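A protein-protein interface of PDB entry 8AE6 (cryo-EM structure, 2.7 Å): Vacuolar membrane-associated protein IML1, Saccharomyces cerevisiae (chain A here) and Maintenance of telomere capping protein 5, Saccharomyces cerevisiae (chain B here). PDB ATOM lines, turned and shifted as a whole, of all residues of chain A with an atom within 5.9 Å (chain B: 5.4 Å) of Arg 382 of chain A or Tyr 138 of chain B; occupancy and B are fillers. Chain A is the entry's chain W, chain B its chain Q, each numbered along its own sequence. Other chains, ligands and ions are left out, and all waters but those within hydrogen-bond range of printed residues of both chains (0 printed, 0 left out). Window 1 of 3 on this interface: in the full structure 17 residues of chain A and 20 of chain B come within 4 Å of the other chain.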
ATOM      1  N   TRP A 290      -1.732  21.258 -15.911  1.00  0.00           N
ATOM      2  CA  TRP A 290      -1.798  19.810 -16.020  1.00  0.00           C
ATOM      3  C   TRP A 290      -0.859  19.272 -17.086  1.00  0.00           C
ATOM      4  O   TRP A 290      -0.910  18.081 -17.400  1.00  0.00           O
ATOM      5  CB  TRP A 290      -3.236  19.367 -16.295  1.00  0.00           C
ATOM      6  CG  TRP A 290      -4.156  19.708 -15.172  1.00  0.00           C
ATOM      7  CD1 TRP A 290      -4.444  18.938 -14.089  1.00  0.00           C
ATOM      8  CD2 TRP A 290      -4.889  20.923 -15.006  1.00  0.00           C
ATOM      9  NE1 TRP A 290      -5.317  19.594 -13.260  1.00  0.00           N
ATOM     10  CE2 TRP A 290      -5.603  20.817 -13.801  1.00  0.00           C
ATOM     11  CE3 TRP A 290      -5.013  22.093 -15.760  1.00  0.00           C
ATOM     12  CZ2 TRP A 290      -6.432  21.831 -13.336  1.00  0.00           C
ATOM     13  CZ3 TRP A 290      -5.834  23.095 -15.295  1.00  0.00           C
ATOM     14  CH2 TRP A 290      -6.534  22.958 -14.096  1.00  0.00           C
ATOM     15  N   GLU A 377      -9.394  23.288  -3.204  1.00  0.00           N
ATOM     16  CA  GLU A 377      -9.912  24.195  -4.219  1.00  0.00           C
ATOM     17  C   GLU A 377      -9.276  23.948  -5.580  1.00  0.00           C
ATOM     18  O   GLU A 377      -9.947  24.112  -6.607  1.00  0.00           O
ATOM     19  CB  GLU A 377      -9.713  25.641  -3.777  1.00  0.00           C
ATOM     20  CG  GLU A 377     -10.601  26.034  -2.610  1.00  0.00           C
ATOM     21  CD  GLU A 377     -12.000  25.459  -2.721  1.00  0.00           C
ATOM     22  OE1 GLU A 377     -12.733  25.846  -3.656  1.00  0.00           O
ATOM     23  OE2 GLU A 377     -12.367  24.621  -1.871  1.00  0.00           O
ATOM     24  N   PHE A 378      -8.008  23.530  -5.617  1.00  0.00           N
ATOM     25  CA  PHE A 378      -7.420  23.178  -6.900  1.00  0.00           C
ATOM     26  C   PHE A 378      -8.030  21.905  -7.464  1.00  0.00           C
ATOM     27  O   PHE A 378      -8.151  21.772  -8.687  1.00  0.00           O
ATOM     28  CB  PHE A 378      -5.904  23.032  -6.792  1.00  0.00           C
ATOM     29  CG  PHE A 378      -5.199  23.208  -8.102  1.00  0.00           C
ATOM     30  CD1 PHE A 378      -4.775  24.460  -8.509  1.00  0.00           C
ATOM     31  CD2 PHE A 378      -4.995  22.131  -8.948  1.00  0.00           C
ATOM     32  CE1 PHE A 378      -4.142  24.631  -9.721  1.00  0.00           C
ATOM     33  CE2 PHE A 378      -4.373  22.298 -10.163  1.00  0.00           C
ATOM     34  CZ  PHE A 378      -3.941  23.548 -10.548  1.00  0.00           C
ATOM     35  N   MET A 379      -8.421  20.961  -6.606  1.00  0.00           N
ATOM     36  CA  MET A 379      -9.111  19.783  -7.120  1.00  0.00           C
ATOM     37  C   MET A 379     -10.530  20.108  -7.571  1.00  0.00           C
ATOM     38  O   MET A 379     -11.068  19.430  -8.453  1.00  0.00           O
ATOM     39  CB  MET A 379      -9.127  18.677  -6.070  1.00  0.00           C
ATOM     40  CG  MET A 379      -7.806  17.950  -5.924  1.00  0.00           C
ATOM     41  SD  MET A 379      -7.336  17.025  -7.391  1.00  0.00           S
ATOM     42  CE  MET A 379      -5.553  17.116  -7.281  1.00  0.00           C
ATOM     43  N   GLU A 380     -11.156  21.131  -6.986  1.00  0.00           N
ATOM     44  CA  GLU A 380     -12.530  21.471  -7.340  1.00  0.00           C
ATOM     45  C   GLU A 380     -12.657  22.490  -8.473  1.00  0.00           C
ATOM     46  O   GLU A 380     -13.771  22.682  -8.980  1.00  0.00           O
ATOM     47  CB  GLU A 380     -13.268  22.006  -6.111  1.00  0.00           C
ATOM     48  CG  GLU A 380     -13.695  20.936  -5.127  1.00  0.00           C
ATOM     49  CD  GLU A 380     -14.542  21.487  -3.999  1.00  0.00           C
ATOM     50  OE1 GLU A 380     -14.884  22.689  -4.042  1.00  0.00           O
ATOM     51  OE2 GLU A 380     -14.872  20.721  -3.069  1.00  0.00           O
ATOM     52  N   ILE A 381     -11.561  23.146  -8.871  1.00  0.00           N
ATOM     53  CA  ILE A 381     -11.657  24.228  -9.854  1.00  0.00           C
ATOM     54  C   ILE A 381     -12.072  23.720 -11.241  1.00  0.00           C
ATOM     55  O   ILE A 381     -12.750  24.442 -11.990  1.00  0.00           O
ATOM     56  CB  ILE A 381     -10.332  25.026  -9.878  1.00  0.00           C
ATOM     57  CG1 ILE A 381     -10.555  26.430 -10.432  1.00  0.00           C
ATOM     58  CG2 ILE A 381      -9.226  24.312 -10.645  1.00  0.00           C
ATOM     59  CD1 ILE A 381     -11.383  27.317  -9.533  1.00  0.00           C
ATOM     60  N   ARG A 382     -11.731  22.474 -11.590  1.00  0.00           N
ATOM     61  CA  ARG A 382     -12.107  21.935 -12.895  1.00  0.00           C
ATOM     62  C   ARG A 382     -13.610  21.716 -12.995  1.00  0.00           C
ATOM     63  O   ARG A 382     -14.225  22.060 -14.010  1.00  0.00           O
ATOM     64  CB  ARG A 382     -11.370  20.626 -13.164  1.00  0.00           C
ATOM     65  CG  ARG A 382      -9.872  20.754 -13.249  1.00  0.00           C
ATOM     66  CD  ARG A 382      -9.293  19.687 -14.154  1.00  0.00           C
ATOM     67  NE  ARG A 382      -9.142  20.169 -15.522  1.00  0.00           N
ATOM     68  CZ  ARG A 382      -8.881  19.394 -16.566  1.00  0.00           C
ATOM     69  NH1 ARG A 382      -8.734  18.085 -16.437  1.00  0.00           N
ATOM     70  NH2 ARG A 382      -8.764  19.946 -17.770  1.00  0.00           N
ATOM     71  N   LYS A 383     -14.213  21.141 -11.953  1.00  0.00           N
ATOM     72  CA  LYS A 383     -15.664  21.015 -11.905  1.00  0.00           C
ATOM     73  C   LYS A 383     -16.336  22.377 -11.824  1.00  0.00           C
ATOM     74  O   LYS A 383     -17.424  22.562 -12.380  1.00  0.00           O
ATOM     75  CB  LYS A 383     -16.077  20.149 -10.717  1.00  0.00           C
ATOM     76  CG  LYS A 383     -17.560  19.818 -10.664  1.00  0.00           C
ATOM     77  CD  LYS A 383     -17.925  19.095  -9.381  1.00  0.00           C
ATOM     78  CE  LYS A 383     -19.149  18.216  -9.579  1.00  0.00           C
ATOM     79  NZ  LYS A 383     -20.087  18.785 -10.586  1.00  0.00           N
ATOM     80  N   ASP A 384     -15.710  23.332 -11.131  1.00  0.00           N
ATOM     81  CA  ASP A 384     -16.300  24.661 -11.003  1.00  0.00           C
ATOM     82  C   ASP A 384     -16.377  25.377 -12.346  1.00  0.00           C
ATOM     83  O   ASP A 384     -17.365  26.064 -12.631  1.00  0.00           O
ATOM     84  CB  ASP A 384     -15.502  25.495 -10.002  1.00  0.00           C
ATOM     85  CG  ASP A 384     -15.802  25.117  -8.566  1.00  0.00           C
ATOM     86  OD1 ASP A 384     -16.806  24.415  -8.330  1.00  0.00           O
ATOM     87  OD2 ASP A 384     -15.030  25.525  -7.671  1.00  0.00           O
ATOM     88  N   LEU A 385     -15.355  25.230 -13.187  1.00  0.00           N
ATOM     89  CA  LEU A 385     -15.293  26.029 -14.406  1.00  0.00           C
ATOM     90  C   LEU A 385     -15.717  25.280 -15.665  1.00  0.00           C
ATOM     91  O   LEU A 385     -16.457  25.830 -16.483  1.00  0.00           O
ATOM     92  CB  LEU A 385     -13.880  26.589 -14.581  1.00  0.00           C
ATOM     93  CG  LEU A 385     -13.574  27.624 -13.508  1.00  0.00           C
ATOM     94  CD1 LEU A 385     -12.097  27.867 -13.431  1.00  0.00           C
ATOM     95  CD2 LEU A 385     -14.309  28.905 -13.808  1.00  0.00           C
ATOM     96  N   LEU A 386     -15.272  24.042 -15.848  1.00  0.00           N
ATOM     97  CA  LEU A 386     -15.512  23.348 -17.107  1.00  0.00           C
ATOM     98  C   LEU A 386     -16.864  22.654 -17.170  1.00  0.00           C
ATOM     99  O   LEU A 386     -17.150  21.987 -18.171  1.00  0.00           O
ATOM    100  CB  LEU A 386     -14.397  22.331 -17.363  1.00  0.00           C
ATOM    101  CG  LEU A 386     -12.993  22.919 -17.501  1.00  0.00           C
ATOM    102  CD1 LEU A 386     -11.989  21.838 -17.835  1.00  0.00           C
ATOM    103  CD2 LEU A 386     -12.967  24.016 -18.550  1.00  0.00           C
ATOM    104  N   ASN A 387     -17.698  22.783 -16.144  1.00  0.00           N
ATOM    105  CA  ASN A 387     -19.055  22.241 -16.142  1.00  0.00           C
ATOM    106  C   ASN A 387     -20.020  23.422 -16.123  1.00  0.00           C
ATOM    107  O   ASN A 387     -20.477  23.851 -15.061  1.00  0.00           O
ATOM    108  CB  ASN A 387     -19.277  21.325 -14.946  1.00  0.00           C
ATOM    109  CG  ASN A 387     -20.043  20.075 -15.303  1.00  0.00           C
ATOM    110  OD1 ASN A 387     -19.955  19.585 -16.427  1.00  0.00           O
ATOM    111  ND2 ASN A 387     -20.797  19.551 -14.348  1.00  0.00           N
ATOM    112  N   ALA A 397     -20.589  19.798 -20.299  1.00  0.00           N
ATOM    113  CA  ALA A 397     -19.144  19.910 -20.142  1.00  0.00           C
ATOM    114  C   ALA A 397     -18.543  20.733 -21.274  1.00  0.00           C
ATOM    115  O   ALA A 397     -18.261  20.202 -22.353  1.00  0.00           O
ATOM    116  CB  ALA A 397     -18.496  18.525 -20.090  1.00  0.00           C
ATOM    117  N   PHE A 401      -9.456  26.153 -20.725  1.00  0.00           N
ATOM    118  CA  PHE A 401      -8.504  27.077 -20.130  1.00  0.00           C
ATOM    119  C   PHE A 401      -7.601  27.661 -21.206  1.00  0.00           C
ATOM    120  O   PHE A 401      -7.183  26.963 -22.136  1.00  0.00           O
ATOM    121  CB  PHE A 401      -7.658  26.369 -19.071  1.00  0.00           C
ATOM    122  CG  PHE A 401      -8.445  25.863 -17.898  1.00  0.00           C
ATOM    123  CD1 PHE A 401      -9.054  26.745 -17.026  1.00  0.00           C
ATOM    124  CD2 PHE A 401      -8.558  24.508 -17.655  1.00  0.00           C
ATOM    125  CE1 PHE A 401      -9.771  26.285 -15.944  1.00  0.00           C
ATOM    126  CE2 PHE A 401      -9.276  24.046 -16.571  1.00  0.00           C
ATOM    127  CZ  PHE A 401      -9.882  24.940 -15.718  1.00  0.00           C
ATOM    128  N   HIS B 113      -8.909  12.856 -25.167  1.00  0.00           N
ATOM    129  CA  HIS B 113      -8.430  13.053 -23.807  1.00  0.00           C
ATOM    130  C   HIS B 113      -6.950  13.425 -23.777  1.00  0.00           C
ATOM    131  O   HIS B 113      -6.200  13.212 -24.731  1.00  0.00           O
ATOM    132  CB  HIS B 113      -8.637  11.780 -22.992  1.00  0.00           C
ATOM    133  CG  HIS B 113      -9.906  11.052 -23.314  1.00  0.00           C
ATOM    134  ND1 HIS B 113     -11.116  11.380 -22.748  1.00  0.00           N
ATOM    135  CD2 HIS B 113     -10.144   9.999 -24.129  1.00  0.00           C
ATOM    136  CE1 HIS B 113     -12.049  10.565 -23.207  1.00  0.00           C
ATOM    137  NE2 HIS B 113     -11.485   9.719 -24.047  1.00  0.00           N
ATOM    138  N   THR B 132     -15.426   6.614 -25.194  1.00  0.00           N
ATOM    139  CA  THR B 132     -14.093   6.420 -24.642  1.00  0.00           C
ATOM    140  C   THR B 132     -14.014   7.056 -23.262  1.00  0.00           C
ATOM    141  O   THR B 132     -14.482   8.183 -23.066  1.00  0.00           O
ATOM    142  CB  THR B 132     -13.015   7.030 -25.546  1.00  0.00           C
ATOM    143  OG1 THR B 132     -13.047   8.458 -25.433  1.00  0.00           O
ATOM    144  CG2 THR B 132     -13.230   6.639 -26.999  1.00  0.00           C
ATOM    145  N   CYS B 133     -13.421   6.338 -22.316  1.00  0.00           N
ATOM    146  CA  CYS B 133     -13.154   6.841 -20.977  1.00  0.00           C
ATOM    147  C   CYS B 133     -11.656   6.782 -20.717  1.00  0.00           C
ATOM    148  O   CYS B 133     -10.931   5.995 -21.329  1.00  0.00           O
ATOM    149  CB  CYS B 133     -13.915   6.041 -19.917  1.00  0.00           C
ATOM    150  SG  CYS B 133     -13.122   4.501 -19.424  1.00  0.00           S
ATOM    151  N   SER B 134     -11.186   7.630 -19.805  1.00  0.00           N
ATOM    152  CA  SER B 134      -9.753   7.840 -19.671  1.00  0.00           C
ATOM    153  C   SER B 134      -9.385   8.191 -18.237  1.00  0.00           C
ATOM    154  O   SER B 134     -10.245   8.382 -17.374  1.00  0.00           O
ATOM    155  CB  SER B 134      -9.281   8.940 -20.613  1.00  0.00           C
ATOM    156  OG  SER B 134     -10.064  10.102 -20.421  1.00  0.00           O
ATOM    157  N   ASP B 136      -7.917  10.945 -17.348  1.00  0.00           N
ATOM    158  CA  ASP B 136      -8.069  12.373 -17.090  1.00  0.00           C
ATOM    159  C   ASP B 136      -9.479  12.765 -16.650  1.00  0.00           C
ATOM    160  O   ASP B 136      -9.813  13.955 -16.724  1.00  0.00           O
ATOM    161  CB  ASP B 136      -7.649  13.186 -18.320  1.00  0.00           C
ATOM    162  CG  ASP B 136      -8.640  13.092 -19.463  1.00  0.00           C
ATOM    163  OD1 ASP B 136      -9.287  12.041 -19.614  1.00  0.00           O
ATOM    164  OD2 ASP B 136      -8.766  14.077 -20.220  1.00  0.00           O
ATOM    165  N   THR B 137     -10.279  11.796 -16.185  1.00  0.00           N
ATOM    166  CA  THR B 137     -11.649  11.988 -15.696  1.00  0.00           C
ATOM    167  C   THR B 137     -12.537  12.619 -16.767  1.00  0.00           C
ATOM    168  O   THR B 137     -13.049  13.725 -16.611  1.00  0.00           O
ATOM    169  CB  THR B 137     -11.680  12.812 -14.401  1.00  0.00           C
ATOM    170  OG1 THR B 137     -11.457  14.194 -14.707  1.00  0.00           O
ATOM    171  CG2 THR B 137     -10.617  12.338 -13.416  1.00  0.00           C
ATOM    172  N   TYR B 138     -12.702  11.893 -17.872  1.00  0.00           N
ATOM    173  CA  TYR B 138     -13.573  12.320 -18.957  1.00  0.00           C
ATOM    174  C   TYR B 138     -14.126  11.101 -19.675  1.00  0.00           C
ATOM    175  O   TYR B 138     -13.409  10.124 -19.894  1.00  0.00           O
ATOM    176  CB  TYR B 138     -12.849  13.215 -19.967  1.00  0.00           C
ATOM    177  CG  TYR B 138     -12.749  14.661 -19.558  1.00  0.00           C
ATOM    178  CD1 TYR B 138     -13.834  15.509 -19.691  1.00  0.00           C
ATOM    179  CD2 TYR B 138     -11.568  15.179 -19.054  1.00  0.00           C
ATOM    180  CE1 TYR B 138     -13.753  16.832 -19.319  1.00  0.00           C
ATOM    181  CE2 TYR B 138     -11.477  16.501 -18.677  1.00  0.00           C
ATOM    182  CZ  TYR B 138     -12.572  17.321 -18.815  1.00  0.00           C
ATOM    183  OH  TYR B 138     -12.486  18.640 -18.446  1.00  0.00           O
ATOM    184  N   VAL B 139     -15.401  11.174 -20.039  1.00  0.00           N
ATOM    185  CA  VAL B 139     -16.037  10.182 -20.898  1.00  0.00           C
ATOM    186  C   VAL B 139     -16.513  10.907 -22.148  1.00  0.00           C
ATOM    187  O   VAL B 139     -17.392  11.773 -22.076  1.00  0.00           O
ATOM    188  CB  VAL B 139     -17.201   9.466 -20.198  1.00  0.00           C
ATOM    189  CG1 VAL B 139     -17.978   8.628 -21.189  1.00  0.00           C
ATOM    190  CG2 VAL B 139     -16.677   8.600 -19.072  1.00  0.00           C
ATOM    191  N   HIS B 140     -15.922  10.560 -23.286  1.00  0.00           N
ATOM    192  CA  HIS B 140     -16.224  11.188 -24.563  1.00  0.00           C
ATOM    193  C   HIS B 140     -16.945  10.191 -25.452  1.00  0.00           C
ATOM    194  O   HIS B 140     -16.509   9.045 -25.584  1.00  0.00           O
ATOM    195  CB  HIS B 140     -14.949  11.668 -25.258  1.00  0.00           C
ATOM    196  CG  HIS B 140     -14.352  12.898 -24.653  1.00  0.00           C
ATOM    197  ND1 HIS B 140     -15.084  13.793 -23.907  1.00  0.00           N
ATOM    198  CD2 HIS B 140     -13.091  13.386 -24.694  1.00  0.00           C
ATOM    199  CE1 HIS B 140     -14.299  14.777 -23.508  1.00  0.00           C
ATOM    200  NE2 HIS B 140     -13.084  14.554 -23.972  1.00  0.00           N
ATOM    201  N   SER B 153     -19.566  15.097 -24.203  1.00  0.00           N
ATOM    202  CA  SER B 153     -18.488  15.100 -23.227  1.00  0.00           C
ATOM    203  C   SER B 153     -19.084  15.161 -21.832  1.00  0.00           C
ATOM    204  O   SER B 153     -20.011  15.937 -21.585  1.00  0.00           O
ATOM    205  CB  SER B 153     -17.541  16.283 -23.452  1.00  0.00           C
ATOM    206  OG  SER B 153     -16.778  16.552 -22.290  1.00  0.00           O
ATOM    207  N   THR B 154     -18.561  14.337 -20.931  1.00  0.00           N
ATOM    208  CA  THR B 154     -18.977  14.361 -19.538  1.00  0.00           C
ATOM    209  C   THR B 154     -17.805  13.925 -18.674  1.00  0.00           C
ATOM    210  O   THR B 154     -16.827  13.353 -19.164  1.00  0.00           O
ATOM    211  CB  THR B 154     -20.192  13.467 -19.285  1.00  0.00           C
ATOM    212  OG1 THR B 154     -20.650  13.668 -17.944  1.00  0.00           O
ATOM    213  CG2 THR B 154     -19.832  12.007 -19.470  1.00  0.00           C
ATOM    214  N   SER B 155     -17.908  14.212 -17.379  1.00  0.00           N
ATOM    215  CA  SER B 155     -16.791  13.994 -16.476  1.00  0.00           C
ATOM    216  C   SER B 155     -17.306  13.683 -15.081  1.00  0.00           C
ATOM    217  O   SER B 155     -18.428  14.036 -14.716  1.00  0.00           O
ATOM    218  CB  SER B 155     -15.875  15.218 -16.436  1.00  0.00           C
ATOM    219  OG  SER B 155     -14.849  15.054 -15.474  1.00  0.00           O
ATOM    220  N   SER B 156     -16.457  13.014 -14.300  1.00  0.00           N
ATOM    221  CA  SER B 156     -16.704  12.820 -12.877  1.00  0.00           C
ATOM    222  C   SER B 156     -15.948  13.809 -12.009  1.00  0.00           C
ATOM    223  O   SER B 156     -16.296  13.967 -10.832  1.00  0.00           O
ATOM    224  CB  SER B 156     -16.326  11.398 -12.457  1.00  0.00           C
ATOM    225  OG  SER B 156     -14.984  11.113 -12.797  1.00  0.00           O
ATOM    226  N   TRP B 157     -14.900  14.431 -12.550  1.00  0.00           N
ATOM    227  CA  TRP B 157     -14.110  15.528 -11.996  1.00  0.00           C
ATOM    228  C   TRP B 157     -13.259  15.147 -10.790  1.00  0.00           C
ATOM    229  O   TRP B 157     -12.476  15.981 -10.326  1.00  0.00           O
ATOM    230  CB  TRP B 157     -14.976  16.736 -11.613  1.00  0.00           C
ATOM    231  CG  TRP B 157     -15.941  17.144 -12.672  1.00  0.00           C
ATOM    232  CD1 TRP B 157     -17.290  16.961 -12.662  1.00  0.00           C
ATOM    233  CD2 TRP B 157     -15.636  17.819 -13.894  1.00  0.00           C
ATOM    234  NE1 TRP B 157     -17.844  17.476 -13.805  1.00  0.00           N
ATOM    235  CE2 TRP B 157     -16.850  18.010 -14.579  1.00  0.00           C
ATOM    236  CE3 TRP B 157     -14.453  18.279 -14.480  1.00  0.00           C
ATOM    237  CZ2 TRP B 157     -16.917  18.637 -15.819  1.00  0.00           C
ATOM    238  CZ3 TRP B 157     -14.521  18.904 -15.710  1.00  0.00           C
ATOM    239  CH2 TRP B 157     -15.744  19.076 -16.365  1.00  0.00           C
ATOM    240  N   ALA B 161     -11.492   7.208 -14.649  1.00  0.00           N
ATOM    241  CA  ALA B 161     -12.453   6.207 -15.082  1.00  0.00           C
ATOM    242  C   ALA B 161     -11.780   4.853 -15.266  1.00  0.00           C
ATOM    243  O   ALA B 161     -10.577   4.759 -15.519  1.00  0.00           O
ATOM    244  CB  ALA B 161     -13.115   6.638 -16.385  1.00  0.00           C
ATOM    245  N   HIS B 178     -15.867   5.313 -11.879  1.00  0.00           N
ATOM    246  CA  HIS B 178     -14.756   6.191 -11.520  1.00  0.00           C
ATOM    247  C   HIS B 178     -14.381   5.898 -10.072  1.00  0.00           C
ATOM    248  O   HIS B 178     -14.911   6.518  -9.148  1.00  0.00           O
ATOM    249  CB  HIS B 178     -15.127   7.656 -11.699  1.00  0.00           C
ATOM    250  CG  HIS B 178     -15.544   8.016 -13.090  1.00  0.00           C
ATOM    251  ND1 HIS B 178     -14.767   8.797 -13.918  1.00  0.00           N
ATOM    252  CD2 HIS B 178     -16.665   7.727 -13.789  1.00  0.00           C
ATOM    253  CE1 HIS B 178     -15.389   8.965 -15.072  1.00  0.00           C
ATOM    254  NE2 HIS B 178     -16.542   8.324 -15.020  1.00  0.00           N
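The side-chain hydroxyl of Ser 134 of chain B lies within hydrogen-bond range of the backbone carbonyl oxygen of Tyr 138 of chain B (3.4 Å).
OG of Ser 155 of chain B sits at hydrogen-bond distance from N of Trp 157 of chain B (3.0 Å).
Arg 382 of chain A touches just these residues of chain B: Tyr 138 and Trp 157.
Of chain A, only Arg 382 and Leu 386 come within 4 Å of Tyr 138 of chain B.
Of the printed residues of chain A, Trp 157 of chain B touches Arg 382 (3.6 Å), Lys 383 (3.5 Å), Leu 386 (3.7 Å) and Asn 387 (3.2 Å).
Printed residues of chain B within 4 Å of Lys 383 of chain A: Trp 157.
Of the printed residues of chain B, Asn 387 of chain A touches Trp 157 (3.2 Å).
Of the printed residues of chain B, Ala 397 of chain A touches Ser 153.
Of the printed residues of chain B, Leu 386 of chain A touches Tyr 138 and Trp 157.
Ile 381 of chain A touches none of the printed residues of chain B.
Glu 377 of chain A touches none of the printed residues of chain B.
The nearest residue of chain B that does not touch Arg 382 of chain A is Asp 136 of chain B (4.3 Å).
The nearest residue of chain A that does not touch Tyr 138 of chain B is Ala 397 of chain A (5.1 Å).
The nearest printed residue of chain B that does not touch Lys 383 of chain A is Ser 156 of chain B (5.3 Å).
Of the 14 printed residues of chain A, 5 touch a printed residue of chain B.
Printed residues of chain A that touch a printed residue of chain B: Arg 382, Lys 383, Leu 386, Asn 387 and Ala 397.
Of the 16 printed residues of chain B, 3 touch a printed residue of chain A.
Among the printed residues, no Asp or Glu carboxylate lies within 4 Å of a Lys or Arg side-chain nitrogen of the other chain.
Among the printed residues, merely in contact across the chains: Arg 382 of chain A with Tyr 138 of chain B, Arg 382 of chain A with Trp 157 of chain B, Lys 383 of chain A with Trp 157 of chain B, Leu 386 of chain A with Tyr 138 of chain B, Leu 386 of chain A with Trp 157 of chain B, Asn 387 of chain A with Trp 157 of chain B and Ala 397 of chain A with Ser 153 of chain B.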
